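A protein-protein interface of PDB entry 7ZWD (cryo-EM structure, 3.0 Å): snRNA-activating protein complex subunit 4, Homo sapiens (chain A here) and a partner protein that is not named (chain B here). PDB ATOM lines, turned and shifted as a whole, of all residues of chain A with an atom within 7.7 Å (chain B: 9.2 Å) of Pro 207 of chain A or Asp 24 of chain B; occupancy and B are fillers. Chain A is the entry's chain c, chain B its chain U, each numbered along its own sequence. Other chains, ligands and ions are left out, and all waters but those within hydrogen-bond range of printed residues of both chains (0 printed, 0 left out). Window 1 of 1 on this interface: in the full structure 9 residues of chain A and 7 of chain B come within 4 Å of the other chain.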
ATOM      1  N   ARG A 200       9.736  -4.843 -17.329  1.00  0.00           N
ATOM      2  CA  ARG A 200       9.089  -6.033 -16.799  1.00  0.00           C
ATOM      3  C   ARG A 200       9.755  -6.489 -15.512  1.00  0.00           C
ATOM      4  O   ARG A 200       9.076  -6.918 -14.572  1.00  0.00           O
ATOM      5  CB  ARG A 200       9.102  -7.153 -17.824  1.00  0.00           C
ATOM      6  CG  ARG A 200       8.241  -8.296 -17.394  1.00  0.00           C
ATOM      7  CD  ARG A 200       6.812  -7.831 -17.300  1.00  0.00           C
ATOM      8  NE  ARG A 200       5.978  -8.747 -16.537  1.00  0.00           N
ATOM      9  CZ  ARG A 200       5.526  -9.906 -16.997  1.00  0.00           C
ATOM     10  NH1 ARG A 200       5.836 -10.304 -18.222  1.00  0.00           N
ATOM     11  NH2 ARG A 200       4.767 -10.672 -16.228  1.00  0.00           N
ATOM     12  N   LEU A 201      11.085  -6.403 -15.446  1.00  0.00           N
ATOM     13  CA  LEU A 201      11.766  -6.724 -14.196  1.00  0.00           C
ATOM     14  C   LEU A 201      11.290  -5.826 -13.068  1.00  0.00           C
ATOM     15  O   LEU A 201      10.985  -6.304 -11.974  1.00  0.00           O
ATOM     16  CB  LEU A 201      13.279  -6.615 -14.348  1.00  0.00           C
ATOM     17  CG  LEU A 201      13.921  -7.765 -15.107  1.00  0.00           C
ATOM     18  CD1 LEU A 201      15.409  -7.528 -15.282  1.00  0.00           C
ATOM     19  CD2 LEU A 201      13.662  -9.051 -14.357  1.00  0.00           C
ATOM     20  N   GLN A 202      11.235  -4.519 -13.308  1.00  0.00           N
ATOM     21  CA  GLN A 202      10.796  -3.622 -12.245  1.00  0.00           C
ATOM     22  C   GLN A 202       9.364  -3.919 -11.829  1.00  0.00           C
ATOM     23  O   GLN A 202       9.042  -3.924 -10.635  1.00  0.00           O
ATOM     24  CB  GLN A 202      10.933  -2.170 -12.685  1.00  0.00           C
ATOM     25  CG  GLN A 202      12.363  -1.753 -12.919  1.00  0.00           C
ATOM     26  CD  GLN A 202      13.233  -1.964 -11.700  1.00  0.00           C
ATOM     27  OE1 GLN A 202      12.801  -1.744 -10.569  1.00  0.00           O
ATOM     28  NE2 GLN A 202      14.469  -2.390 -11.923  1.00  0.00           N
ATOM     29  N   ARG A 203       8.488  -4.174 -12.800  1.00  0.00           N
ATOM     30  CA  ARG A 203       7.090  -4.424 -12.479  1.00  0.00           C
ATOM     31  C   ARG A 203       6.933  -5.715 -11.694  1.00  0.00           C
ATOM     32  O   ARG A 203       6.073  -5.812 -10.813  1.00  0.00           O
ATOM     33  CB  ARG A 203       6.255  -4.463 -13.759  1.00  0.00           C
ATOM     34  CG  ARG A 203       5.011  -5.326 -13.665  1.00  0.00           C
ATOM     35  CD  ARG A 203       3.838  -4.705 -14.395  1.00  0.00           C
ATOM     36  NE  ARG A 203       3.383  -3.485 -13.732  1.00  0.00           N
ATOM     37  CZ  ARG A 203       2.192  -2.927 -13.920  1.00  0.00           C
ATOM     38  NH1 ARG A 203       1.874  -1.813 -13.278  1.00  0.00           N
ATOM     39  NH2 ARG A 203       1.315  -3.486 -14.742  1.00  0.00           N
ATOM     40  N   LEU A 204       7.757  -6.716 -11.988  1.00  0.00           N
ATOM     41  CA  LEU A 204       7.667  -7.960 -11.238  1.00  0.00           C
ATOM     42  C   LEU A 204       8.343  -7.858  -9.878  1.00  0.00           C
ATOM     43  O   LEU A 204       7.958  -8.569  -8.945  1.00  0.00           O
ATOM     44  CB  LEU A 204       8.272  -9.101 -12.044  1.00  0.00           C
ATOM     45  CG  LEU A 204       7.284  -9.748 -13.003  1.00  0.00           C
ATOM     46  CD1 LEU A 204       7.920 -10.927 -13.697  1.00  0.00           C
ATOM     47  CD2 LEU A 204       6.050 -10.178 -12.243  1.00  0.00           C
ATOM     48  N   LEU A 205       9.334  -6.983  -9.741  1.00  0.00           N
ATOM     49  CA  LEU A 205      10.056  -6.883  -8.481  1.00  0.00           C
ATOM     50  C   LEU A 205       9.297  -6.050  -7.466  1.00  0.00           C
ATOM     51  O   LEU A 205       9.283  -6.386  -6.278  1.00  0.00           O
ATOM     52  CB  LEU A 205      11.433  -6.277  -8.715  1.00  0.00           C
ATOM     53  CG  LEU A 205      12.481  -7.266  -9.191  1.00  0.00           C
ATOM     54  CD1 LEU A 205      13.859  -6.655  -9.081  1.00  0.00           C
ATOM     55  CD2 LEU A 205      12.378  -8.521  -8.373  1.00  0.00           C
ATOM     56  N   GLN A 206       8.673  -4.960  -7.912  1.00  0.00           N
ATOM     57  CA  GLN A 206       8.004  -4.038  -6.997  1.00  0.00           C
ATOM     58  C   GLN A 206       7.086  -4.721  -5.993  1.00  0.00           C
ATOM     59  O   GLN A 206       7.176  -4.396  -4.797  1.00  0.00           O
ATOM     60  CB  GLN A 206       7.241  -2.990  -7.815  1.00  0.00           C
ATOM     61  CG  GLN A 206       8.100  -1.827  -8.247  1.00  0.00           C
ATOM     62  CD  GLN A 206       8.535  -0.972  -7.082  1.00  0.00           C
ATOM     63  OE1 GLN A 206       9.532  -1.261  -6.424  1.00  0.00           O
ATOM     64  NE2 GLN A 206       7.788   0.091  -6.820  1.00  0.00           N
ATOM     65  N   PRO A 207       6.216  -5.662  -6.376  1.00  0.00           N
ATOM     66  CA  PRO A 207       5.393  -6.317  -5.348  1.00  0.00           C
ATOM     67  C   PRO A 207       6.225  -7.045  -4.311  1.00  0.00           C
ATOM     68  O   PRO A 207       6.036  -6.842  -3.107  1.00  0.00           O
ATOM     69  CB  PRO A 207       4.518  -7.282  -6.160  1.00  0.00           C
ATOM     70  CG  PRO A 207       4.569  -6.783  -7.541  1.00  0.00           C
ATOM     71  CD  PRO A 207       5.928  -6.211  -7.709  1.00  0.00           C
ATOM     72  N   LYS A 208       7.157  -7.887  -4.752  1.00  0.00           N
ATOM     73  CA  LYS A 208       7.943  -8.661  -3.805  1.00  0.00           C
ATOM     74  C   LYS A 208       8.875  -7.778  -2.990  1.00  0.00           C
ATOM     75  O   LYS A 208       9.099  -8.050  -1.807  1.00  0.00           O
ATOM     76  CB  LYS A 208       8.723  -9.740  -4.540  1.00  0.00           C
ATOM     77  CG  LYS A 208       8.041 -11.084  -4.514  1.00  0.00           C
ATOM     78  CD  LYS A 208       6.788 -11.078  -5.359  1.00  0.00           C
ATOM     79  CE  LYS A 208       6.069 -12.408  -5.265  1.00  0.00           C
ATOM     80  NZ  LYS A 208       4.996 -12.529  -6.284  1.00  0.00           N
ATOM     81  N   LEU A 209       9.420  -6.721  -3.590  1.00  0.00           N
ATOM     82  CA  LEU A 209      10.214  -5.777  -2.812  1.00  0.00           C
ATOM     83  C   LEU A 209       9.383  -5.145  -1.710  1.00  0.00           C
ATOM     84  O   LEU A 209       9.840  -5.021  -0.567  1.00  0.00           O
ATOM     85  CB  LEU A 209      10.793  -4.696  -3.717  1.00  0.00           C
ATOM     86  CG  LEU A 209      12.213  -4.922  -4.224  1.00  0.00           C
ATOM     87  CD1 LEU A 209      13.179  -4.818  -3.066  1.00  0.00           C
ATOM     88  CD2 LEU A 209      12.339  -6.268  -4.901  1.00  0.00           C
ATOM     89  N   LEU A 210       8.155  -4.742  -2.031  1.00  0.00           N
ATOM     90  CA  LEU A 210       7.305  -4.138  -1.015  1.00  0.00           C
ATOM     91  C   LEU A 210       6.944  -5.149   0.064  1.00  0.00           C
ATOM     92  O   LEU A 210       6.889  -4.806   1.249  1.00  0.00           O
ATOM     93  CB  LEU A 210       6.048  -3.567  -1.663  1.00  0.00           C
ATOM     94  CG  LEU A 210       5.020  -2.951  -0.721  1.00  0.00           C
ATOM     95  CD1 LEU A 210       5.693  -2.031   0.276  1.00  0.00           C
ATOM     96  CD2 LEU A 210       3.966  -2.202  -1.509  1.00  0.00           C
ATOM     97  N   LYS A 211       6.703  -6.400  -0.325  1.00  0.00           N
ATOM     98  CA  LYS A 211       6.411  -7.436   0.660  1.00  0.00           C
ATOM     99  C   LYS A 211       7.590  -7.651   1.595  1.00  0.00           C
ATOM    100  O   LYS A 211       7.412  -7.794   2.811  1.00  0.00           O
ATOM    101  CB  LYS A 211       6.047  -8.735  -0.049  1.00  0.00           C
ATOM    102  CG  LYS A 211       5.797  -9.911   0.867  1.00  0.00           C
ATOM    103  CD  LYS A 211       5.439 -11.141   0.048  1.00  0.00           C
ATOM    104  CE  LYS A 211       5.080 -12.329   0.923  1.00  0.00           C
ATOM    105  NZ  LYS A 211       6.254 -12.837   1.679  1.00  0.00           N
ATOM    106  N   LEU A 212       8.802  -7.679   1.044  1.00  0.00           N
ATOM    107  CA  LEU A 212       9.993  -7.840   1.867  1.00  0.00           C
ATOM    108  C   LEU A 212      10.153  -6.676   2.833  1.00  0.00           C
ATOM    109  O   LEU A 212      10.448  -6.874   4.019  1.00  0.00           O
ATOM    110  CB  LEU A 212      11.220  -7.965   0.971  1.00  0.00           C
ATOM    111  CG  LEU A 212      12.517  -8.411   1.631  1.00  0.00           C
ATOM    112  CD1 LEU A 212      12.314  -9.763   2.277  1.00  0.00           C
ATOM    113  CD2 LEU A 212      13.629  -8.467   0.604  1.00  0.00           C
ATOM    114  N   GLU A 213       9.956  -5.452   2.345  1.00  0.00           N
ATOM    115  CA  GLU A 213      10.066  -4.292   3.220  1.00  0.00           C
ATOM    116  C   GLU A 213       9.010  -4.334   4.316  1.00  0.00           C
ATOM    117  O   GLU A 213       9.279  -3.966   5.465  1.00  0.00           O
ATOM    118  CB  GLU A 213       9.954  -3.010   2.397  1.00  0.00           C
ATOM    119  CG  GLU A 213      10.638  -1.795   3.008  1.00  0.00           C
ATOM    120  CD  GLU A 213       9.959  -1.289   4.264  1.00  0.00           C
ATOM    121  OE1 GLU A 213       8.719  -1.402   4.362  1.00  0.00           O
ATOM    122  OE2 GLU A 213      10.666  -0.778   5.157  1.00  0.00           O
ATOM    123  N   TYR A 214       7.800  -4.788   3.983  1.00  0.00           N
ATOM    124  CA  TYR A 214       6.740  -4.869   4.980  1.00  0.00           C
ATOM    125  C   TYR A 214       7.059  -5.915   6.035  1.00  0.00           C
ATOM    126  O   TYR A 214       6.790  -5.714   7.227  1.00  0.00           O
ATOM    127  CB  TYR A 214       5.414  -5.185   4.300  1.00  0.00           C
ATOM    128  CG  TYR A 214       4.235  -5.203   5.233  1.00  0.00           C
ATOM    129  CD1 TYR A 214       3.912  -4.092   5.992  1.00  0.00           C
ATOM    130  CD2 TYR A 214       3.439  -6.330   5.348  1.00  0.00           C
ATOM    131  CE1 TYR A 214       2.828  -4.102   6.844  1.00  0.00           C
ATOM    132  CE2 TYR A 214       2.353  -6.352   6.196  1.00  0.00           C
ATOM    133  CZ  TYR A 214       2.053  -5.235   6.942  1.00  0.00           C
ATOM    134  OH  TYR A 214       0.972  -5.256   7.789  1.00  0.00           O
ATOM    135  N   ILE A 242      12.320 -13.227  -4.813  1.00  0.00           N
ATOM    136  CA  ILE A 242      12.974 -12.130  -5.520  1.00  0.00           C
ATOM    137  C   ILE A 242      14.180 -12.643  -6.293  1.00  0.00           C
ATOM    138  O   ILE A 242      14.485 -12.168  -7.393  1.00  0.00           O
ATOM    139  CB  ILE A 242      13.359 -11.009  -4.541  1.00  0.00           C
ATOM    140  CG1 ILE A 242      12.103 -10.336  -4.003  1.00  0.00           C
ATOM    141  CG2 ILE A 242      14.254  -9.990  -5.206  1.00  0.00           C
ATOM    142  CD1 ILE A 242      12.366  -9.349  -2.898  1.00  0.00           C
ATOM    143  N   ILE A 245      12.935 -14.321  -9.398  1.00  0.00           N
ATOM    144  CA  ILE A 245      12.499 -13.323 -10.366  1.00  0.00           C
ATOM    145  C   ILE A 245      13.699 -12.668 -11.037  1.00  0.00           C
ATOM    146  O   ILE A 245      13.696 -12.435 -12.251  1.00  0.00           O
ATOM    147  CB  ILE A 245      11.587 -12.293  -9.683  1.00  0.00           C
ATOM    148  CG1 ILE A 245      10.249 -12.941  -9.342  1.00  0.00           C
ATOM    149  CG2 ILE A 245      11.388 -11.091 -10.570  1.00  0.00           C
ATOM    150  CD1 ILE A 245       9.248 -11.989  -8.756  1.00  0.00           C
ATOM    151  N   SER B  16      -3.114   4.747 -14.593  1.00  0.00           N
ATOM    152  CA  SER B  16      -1.805   4.129 -14.422  1.00  0.00           C
ATOM    153  C   SER B  16      -1.411   4.073 -12.956  1.00  0.00           C
ATOM    154  O   SER B  16      -0.915   3.052 -12.472  1.00  0.00           O
ATOM    155  CB  SER B  16      -0.758   4.898 -15.218  1.00  0.00           C
ATOM    156  OG  SER B  16       0.533   4.389 -14.954  1.00  0.00           O
ATOM    157  N   VAL B  17      -1.613   5.174 -12.236  1.00  0.00           N
ATOM    158  CA  VAL B  17      -1.269   5.209 -10.819  1.00  0.00           C
ATOM    159  C   VAL B  17      -2.105   4.205 -10.046  1.00  0.00           C
ATOM    160  O   VAL B  17      -1.595   3.487  -9.179  1.00  0.00           O
ATOM    161  CB  VAL B  17      -1.450   6.631 -10.265  1.00  0.00           C
ATOM    162  CG1 VAL B  17      -1.426   6.610  -8.760  1.00  0.00           C
ATOM    163  CG2 VAL B  17      -0.375   7.538 -10.799  1.00  0.00           C
ATOM    164  N   ILE B  18      -3.401   4.142 -10.340  1.00  0.00           N
ATOM    165  CA  ILE B  18      -4.273   3.202  -9.644  1.00  0.00           C
ATOM    166  C   ILE B  18      -3.815   1.775  -9.889  1.00  0.00           C
ATOM    167  O   ILE B  18      -3.729   0.966  -8.959  1.00  0.00           O
ATOM    168  CB  ILE B  18      -5.729   3.405 -10.085  1.00  0.00           C
ATOM    169  CG1 ILE B  18      -6.243   4.755  -9.611  1.00  0.00           C
ATOM    170  CG2 ILE B  18      -6.597   2.308  -9.532  1.00  0.00           C
ATOM    171  CD1 ILE B  18      -7.589   5.101 -10.170  1.00  0.00           C
ATOM    172  N   GLU B  19      -3.514   1.445 -11.143  1.00  0.00           N
ATOM    173  CA  GLU B  19      -3.100   0.086 -11.465  1.00  0.00           C
ATOM    174  C   GLU B  19      -1.767  -0.250 -10.817  1.00  0.00           C
ATOM    175  O   GLU B  19      -1.575  -1.370 -10.338  1.00  0.00           O
ATOM    176  CB  GLU B  19      -3.027  -0.095 -12.975  1.00  0.00           C
ATOM    177  CG  GLU B  19      -4.338  -0.521 -13.598  1.00  0.00           C
ATOM    178  CD  GLU B  19      -4.411  -0.205 -15.075  1.00  0.00           C
ATOM    179  OE1 GLU B  19      -3.449  -0.525 -15.807  1.00  0.00           O
ATOM    180  OE2 GLU B  19      -5.435   0.361 -15.510  1.00  0.00           O
ATOM    181  N   ASP B  20      -0.840   0.706 -10.778  1.00  0.00           N
ATOM    182  CA  ASP B  20       0.433   0.467 -10.110  1.00  0.00           C
ATOM    183  C   ASP B  20       0.230   0.208  -8.626  1.00  0.00           C
ATOM    184  O   ASP B  20       0.790  -0.740  -8.068  1.00  0.00           O
ATOM    185  CB  ASP B  20       1.365   1.655 -10.312  1.00  0.00           C
ATOM    186  CG  ASP B  20       2.326   1.451 -11.456  1.00  0.00           C
ATOM    187  OD1 ASP B  20       2.501   0.296 -11.891  1.00  0.00           O
ATOM    188  OD2 ASP B  20       2.917   2.449 -11.912  1.00  0.00           O
ATOM    189  N   VAL B  21      -0.567   1.047  -7.966  1.00  0.00           N
ATOM    190  CA  VAL B  21      -0.781   0.884  -6.534  1.00  0.00           C
ATOM    191  C   VAL B  21      -1.451  -0.448  -6.242  1.00  0.00           C
ATOM    192  O   VAL B  21      -1.091  -1.139  -5.284  1.00  0.00           O
ATOM    193  CB  VAL B  21      -1.595   2.062  -5.980  1.00  0.00           C
ATOM    194  CG1 VAL B  21      -2.093   1.750  -4.589  1.00  0.00           C
ATOM    195  CG2 VAL B  21      -0.749   3.308  -5.965  1.00  0.00           C
ATOM    196  N   ILE B  22      -2.419  -0.844  -7.067  1.00  0.00           N
ATOM    197  CA  ILE B  22      -3.096  -2.114  -6.834  1.00  0.00           C
ATOM    198  C   ILE B  22      -2.152  -3.280  -7.084  1.00  0.00           C
ATOM    199  O   ILE B  22      -2.146  -4.262  -6.335  1.00  0.00           O
ATOM    200  CB  ILE B  22      -4.358  -2.209  -7.703  1.00  0.00           C
ATOM    201  CG1 ILE B  22      -5.442  -1.291  -7.141  1.00  0.00           C
ATOM    202  CG2 ILE B  22      -4.836  -3.643  -7.797  1.00  0.00           C
ATOM    203  CD1 ILE B  22      -5.674  -1.461  -5.662  1.00  0.00           C
ATOM    204  N   ASN B  23      -1.327  -3.188  -8.123  1.00  0.00           N
ATOM    205  CA  ASN B  23      -0.403  -4.267  -8.431  1.00  0.00           C
ATOM    206  C   ASN B  23       0.678  -4.407  -7.370  1.00  0.00           C
ATOM    207  O   ASN B  23       1.143  -5.521  -7.110  1.00  0.00           O
ATOM    208  CB  ASN B  23       0.223  -4.031  -9.800  1.00  0.00           C
ATOM    209  CG  ASN B  23       1.472  -4.843 -10.013  1.00  0.00           C
ATOM    210  OD1 ASN B  23       1.407  -6.023 -10.349  1.00  0.00           O
ATOM    211  ND2 ASN B  23       2.624  -4.214  -9.826  1.00  0.00           N
ATOM    212  N   ASP B  24       1.088  -3.308  -6.746  1.00  0.00           N
ATOM    213  CA  ASP B  24       2.192  -3.364  -5.798  1.00  0.00           C
ATOM    214  C   ASP B  24       1.764  -3.759  -4.394  1.00  0.00           C
ATOM    215  O   ASP B  24       2.583  -4.283  -3.636  1.00  0.00           O
ATOM    216  CB  ASP B  24       2.910  -2.017  -5.747  1.00  0.00           C
ATOM    217  CG  ASP B  24       3.446  -1.602  -7.093  1.00  0.00           C
ATOM    218  OD1 ASP B  24       3.274  -2.373  -8.059  1.00  0.00           O
ATOM    219  OD2 ASP B  24       4.041  -0.509  -7.189  1.00  0.00           O
ATOM    220  N   VAL B  25       0.505  -3.523  -4.017  1.00  0.00           N
ATOM    221  CA  VAL B  25       0.054  -3.896  -2.684  1.00  0.00           C
ATOM    222  C   VAL B  25      -0.671  -5.228  -2.667  1.00  0.00           C
ATOM    223  O   VAL B  25      -1.108  -5.670  -1.597  1.00  0.00           O
ATOM    224  CB  VAL B  25      -0.859  -2.816  -2.077  1.00  0.00           C
ATOM    225  CG1 VAL B  25      -0.210  -1.459  -2.202  1.00  0.00           C
ATOM    226  CG2 VAL B  25      -2.213  -2.836  -2.749  1.00  0.00           C
ATOM    227  N   ARG B  26      -0.819  -5.882  -3.819  1.00  0.00           N
ATOM    228  CA  ARG B  26      -1.488  -7.177  -3.860  1.00  0.00           C
ATOM    229  C   ARG B  26      -0.844  -8.162  -2.895  1.00  0.00           C
ATOM    230  O   ARG B  26      -1.539  -8.916  -2.200  1.00  0.00           O
ATOM    231  CB  ARG B  26      -1.453  -7.721  -5.283  1.00  0.00           C
ATOM    232  CG  ARG B  26      -2.045  -9.090  -5.449  1.00  0.00           C
ATOM    233  CD  ARG B  26      -2.294  -9.355  -6.912  1.00  0.00           C
ATOM    234  NE  ARG B  26      -3.175  -8.346  -7.487  1.00  0.00           N
ATOM    235  CZ  ARG B  26      -3.215  -8.039  -8.778  1.00  0.00           C
ATOM    236  NH1 ARG B  26      -2.414  -8.657  -9.633  1.00  0.00           N
ATOM    237  NH2 ARG B  26      -4.052  -7.110  -9.213  1.00  0.00           N
ATOM    238  N   ASP B  27       0.484  -8.151  -2.823  1.00  0.00           N
ATOM    239  CA  ASP B  27       1.192  -9.112  -1.990  1.00  0.00           C
ATOM    240  C   ASP B  27       0.954  -8.850  -0.509  1.00  0.00           C
ATOM    241  O   ASP B  27       0.849  -9.794   0.275  1.00  0.00           O
ATOM    242  CB  ASP B  27       2.677  -9.062  -2.306  1.00  0.00           C
ATOM    243  CG  ASP B  27       3.240  -7.684  -2.123  1.00  0.00           C
ATOM    244  OD1 ASP B  27       3.460  -7.280  -0.964  1.00  0.00           O
ATOM    245  OD2 ASP B  27       3.395  -6.980  -3.134  1.00  0.00           O
ATOM    246  N   ILE B  28       0.882  -7.580  -0.100  1.00  0.00           N
ATOM    247  CA  ILE B  28       0.605  -7.293   1.304  1.00  0.00           C
ATOM    248  C   ILE B  28      -0.776  -7.799   1.682  1.00  0.00           C
ATOM    249  O   ILE B  28      -0.971  -8.390   2.752  1.00  0.00           O
ATOM    250  CB  ILE B  28       0.735  -5.790   1.597  1.00  0.00           C
ATOM    251  CG1 ILE B  28       1.943  -5.193   0.895  1.00  0.00           C
ATOM    252  CG2 ILE B  28       0.866  -5.568   3.080  1.00  0.00           C
ATOM    253  CD1 ILE B  28       2.201  -3.768   1.306  1.00  0.00           C
ATOM    254  N   PHE B  29      -1.761  -7.559   0.816  1.00  0.00           N
ATOM    255  CA  PHE B  29      -3.110  -8.041   1.075  1.00  0.00           C
ATOM    256  C   PHE B  29      -3.126  -9.558   1.188  1.00  0.00           C
ATOM    257  O   PHE B  29      -3.766 -10.121   2.083  1.00  0.00           O
ATOM    258  CB  PHE B  29      -4.050  -7.570  -0.030  1.00  0.00           C
ATOM    259  CG  PHE B  29      -4.507  -6.153   0.126  1.00  0.00           C
ATOM    260  CD1 PHE B  29      -3.592  -5.121   0.192  1.00  0.00           C
ATOM    261  CD2 PHE B  29      -5.852  -5.851   0.190  1.00  0.00           C
ATOM    262  CE1 PHE B  29      -4.007  -3.817   0.329  1.00  0.00           C
ATOM    263  CE2 PHE B  29      -6.275  -4.548   0.326  1.00  0.00           C
ATOM    264  CZ  PHE B  29      -5.350  -3.531   0.396  1.00  0.00           C
ATOM    265  N   LEU B  30      -2.417 -10.236   0.284  1.00  0.00           N
ATOM    266  CA  LEU B  30      -2.271 -11.683   0.394  1.00  0.00           C
ATOM    267  C   LEU B  30      -1.623 -12.076   1.716  1.00  0.00           C
ATOM    268  O   LEU B  30      -2.041 -13.049   2.355  1.00  0.00           O
ATOM    269  CB  LEU B  30      -1.456 -12.205  -0.790  1.00  0.00           C
ATOM    270  CG  LEU B  30      -0.871 -13.618  -0.751  1.00  0.00           C
ATOM    271  CD1 LEU B  30      -0.847 -14.199  -2.149  1.00  0.00           C
ATOM    272  CD2 LEU B  30       0.543 -13.608  -0.184  1.00  0.00           C
ATOM    273  N   ASP B  31      -0.610 -11.323   2.143  1.00  0.00           N
ATOM    274  CA  ASP B  31       0.202 -11.715   3.288  1.00  0.00           C
ATOM    275  C   ASP B  31      -0.572 -11.584   4.590  1.00  0.00           C
ATOM    276  O   ASP B  31      -0.756 -12.564   5.319  1.00  0.00           O
ATOM    277  CB  ASP B  31       1.472 -10.866   3.332  1.00  0.00           C
ATOM    278  CG  ASP B  31       2.303 -11.122   4.569  1.00  0.00           C
ATOM    279  OD1 ASP B  31       2.224 -12.239   5.123  1.00  0.00           O
ATOM    280  OD2 ASP B  31       3.033 -10.203   4.995  1.00  0.00           O
ATOM    281  N   LEU B  39      -9.248  -6.390  -2.400  1.00  0.00           N
ATOM    282  CA  LEU B  39      -8.370  -5.569  -3.223  1.00  0.00           C
ATOM    283  C   LEU B  39      -9.099  -5.036  -4.449  1.00  0.00           C
ATOM    284  O   LEU B  39      -8.992  -3.848  -4.777  1.00  0.00           O
ATOM    285  CB  LEU B  39      -7.146  -6.377  -3.642  1.00  0.00           C
ATOM    286  CG  LEU B  39      -6.076  -5.599  -4.391  1.00  0.00           C
ATOM    287  CD1 LEU B  39      -5.461  -4.575  -3.467  1.00  0.00           C
ATOM    288  CD2 LEU B  39      -5.024  -6.547  -4.919  1.00  0.00           C
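OD1 of Asp 20 of chain B lies within salt-bridge range of NH1 of Arg 203 of chain A (2.6 Å). O of Pro 207 of chain A sits close to OD2 of Asp 27 of chain B (2.6 Å). The side-chain carboxylate of Asp 27 of chain B sits close to the backbone NH of Lys 211 of chain A (3.4 Å).
OD1 of Asp 24 of chain B is in hydrogen-bond range of ND2 of Asn 23 of chain B (2.6 Å).
O of Arg 203 of chain A touches ND2 of Asn 23 of chain B, 3.9 Å away. NE2 of Gln 206 of chain A touches OD2 of Asp 24 of chain B (3.8 Å). Asn 23 of chain B touches Pro 207 of chain A. Asp 24 of chain B touches Pro 207 of chain A (O to CA, 3.9 Å). Asp 24 of chain B touches Leu 210 of chain A. CD1 of Ile 28 of chain B touches CG of Leu 210 of chain A (3.6 Å). Tyr 214 of chain A touches Ile 28 of chain B (CD2 to CG2, 3.5 Å). Tyr 214 of chain A touches Asp 31 of chain B.
Printed residues of chain B within 4 Å of Gln 206 of chain A: Asp 24. Of the printed residues of chain B, Lys 211 of chain A touches Asp 27 (3.1 Å). Of chain A, only Gln 206, Pro 207 and Leu 210 come within 4 Å of Asp 24 of chain B. Of the printed residues of chain A, Ile 28 of chain B touches Leu 210 (3.6 Å) and Tyr 214 (3.5 Å). Phe 29 of chain B touches none of the printed residues of chain A. Printed residues of chain A within 4 Å of Asp 31 of chain B: Tyr 214. The nearest residue of chain A that does not touch Asp 24 of chain B is Arg 203 of chain A (5.2 Å). The nearest printed residue of chain A that does not touch Asp 20 of chain B is Gln 206 of chain A (6.8 Å).
Of the 17 printed residues of chain B, 6 touch a printed residue of chain A. Of the 17 printed residues of chain A, 6 touch a printed residue of chain B. Along chain A the printed residues that touch a printed residue of chain B span positions 203 to 214. Among the printed residues, Asp or Glu carboxylates within 4 Å of a Lys or Arg side-chain nitrogen of the other chain: Arg 203 of chain A with Asp 20 of chain B (2.6 Å).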
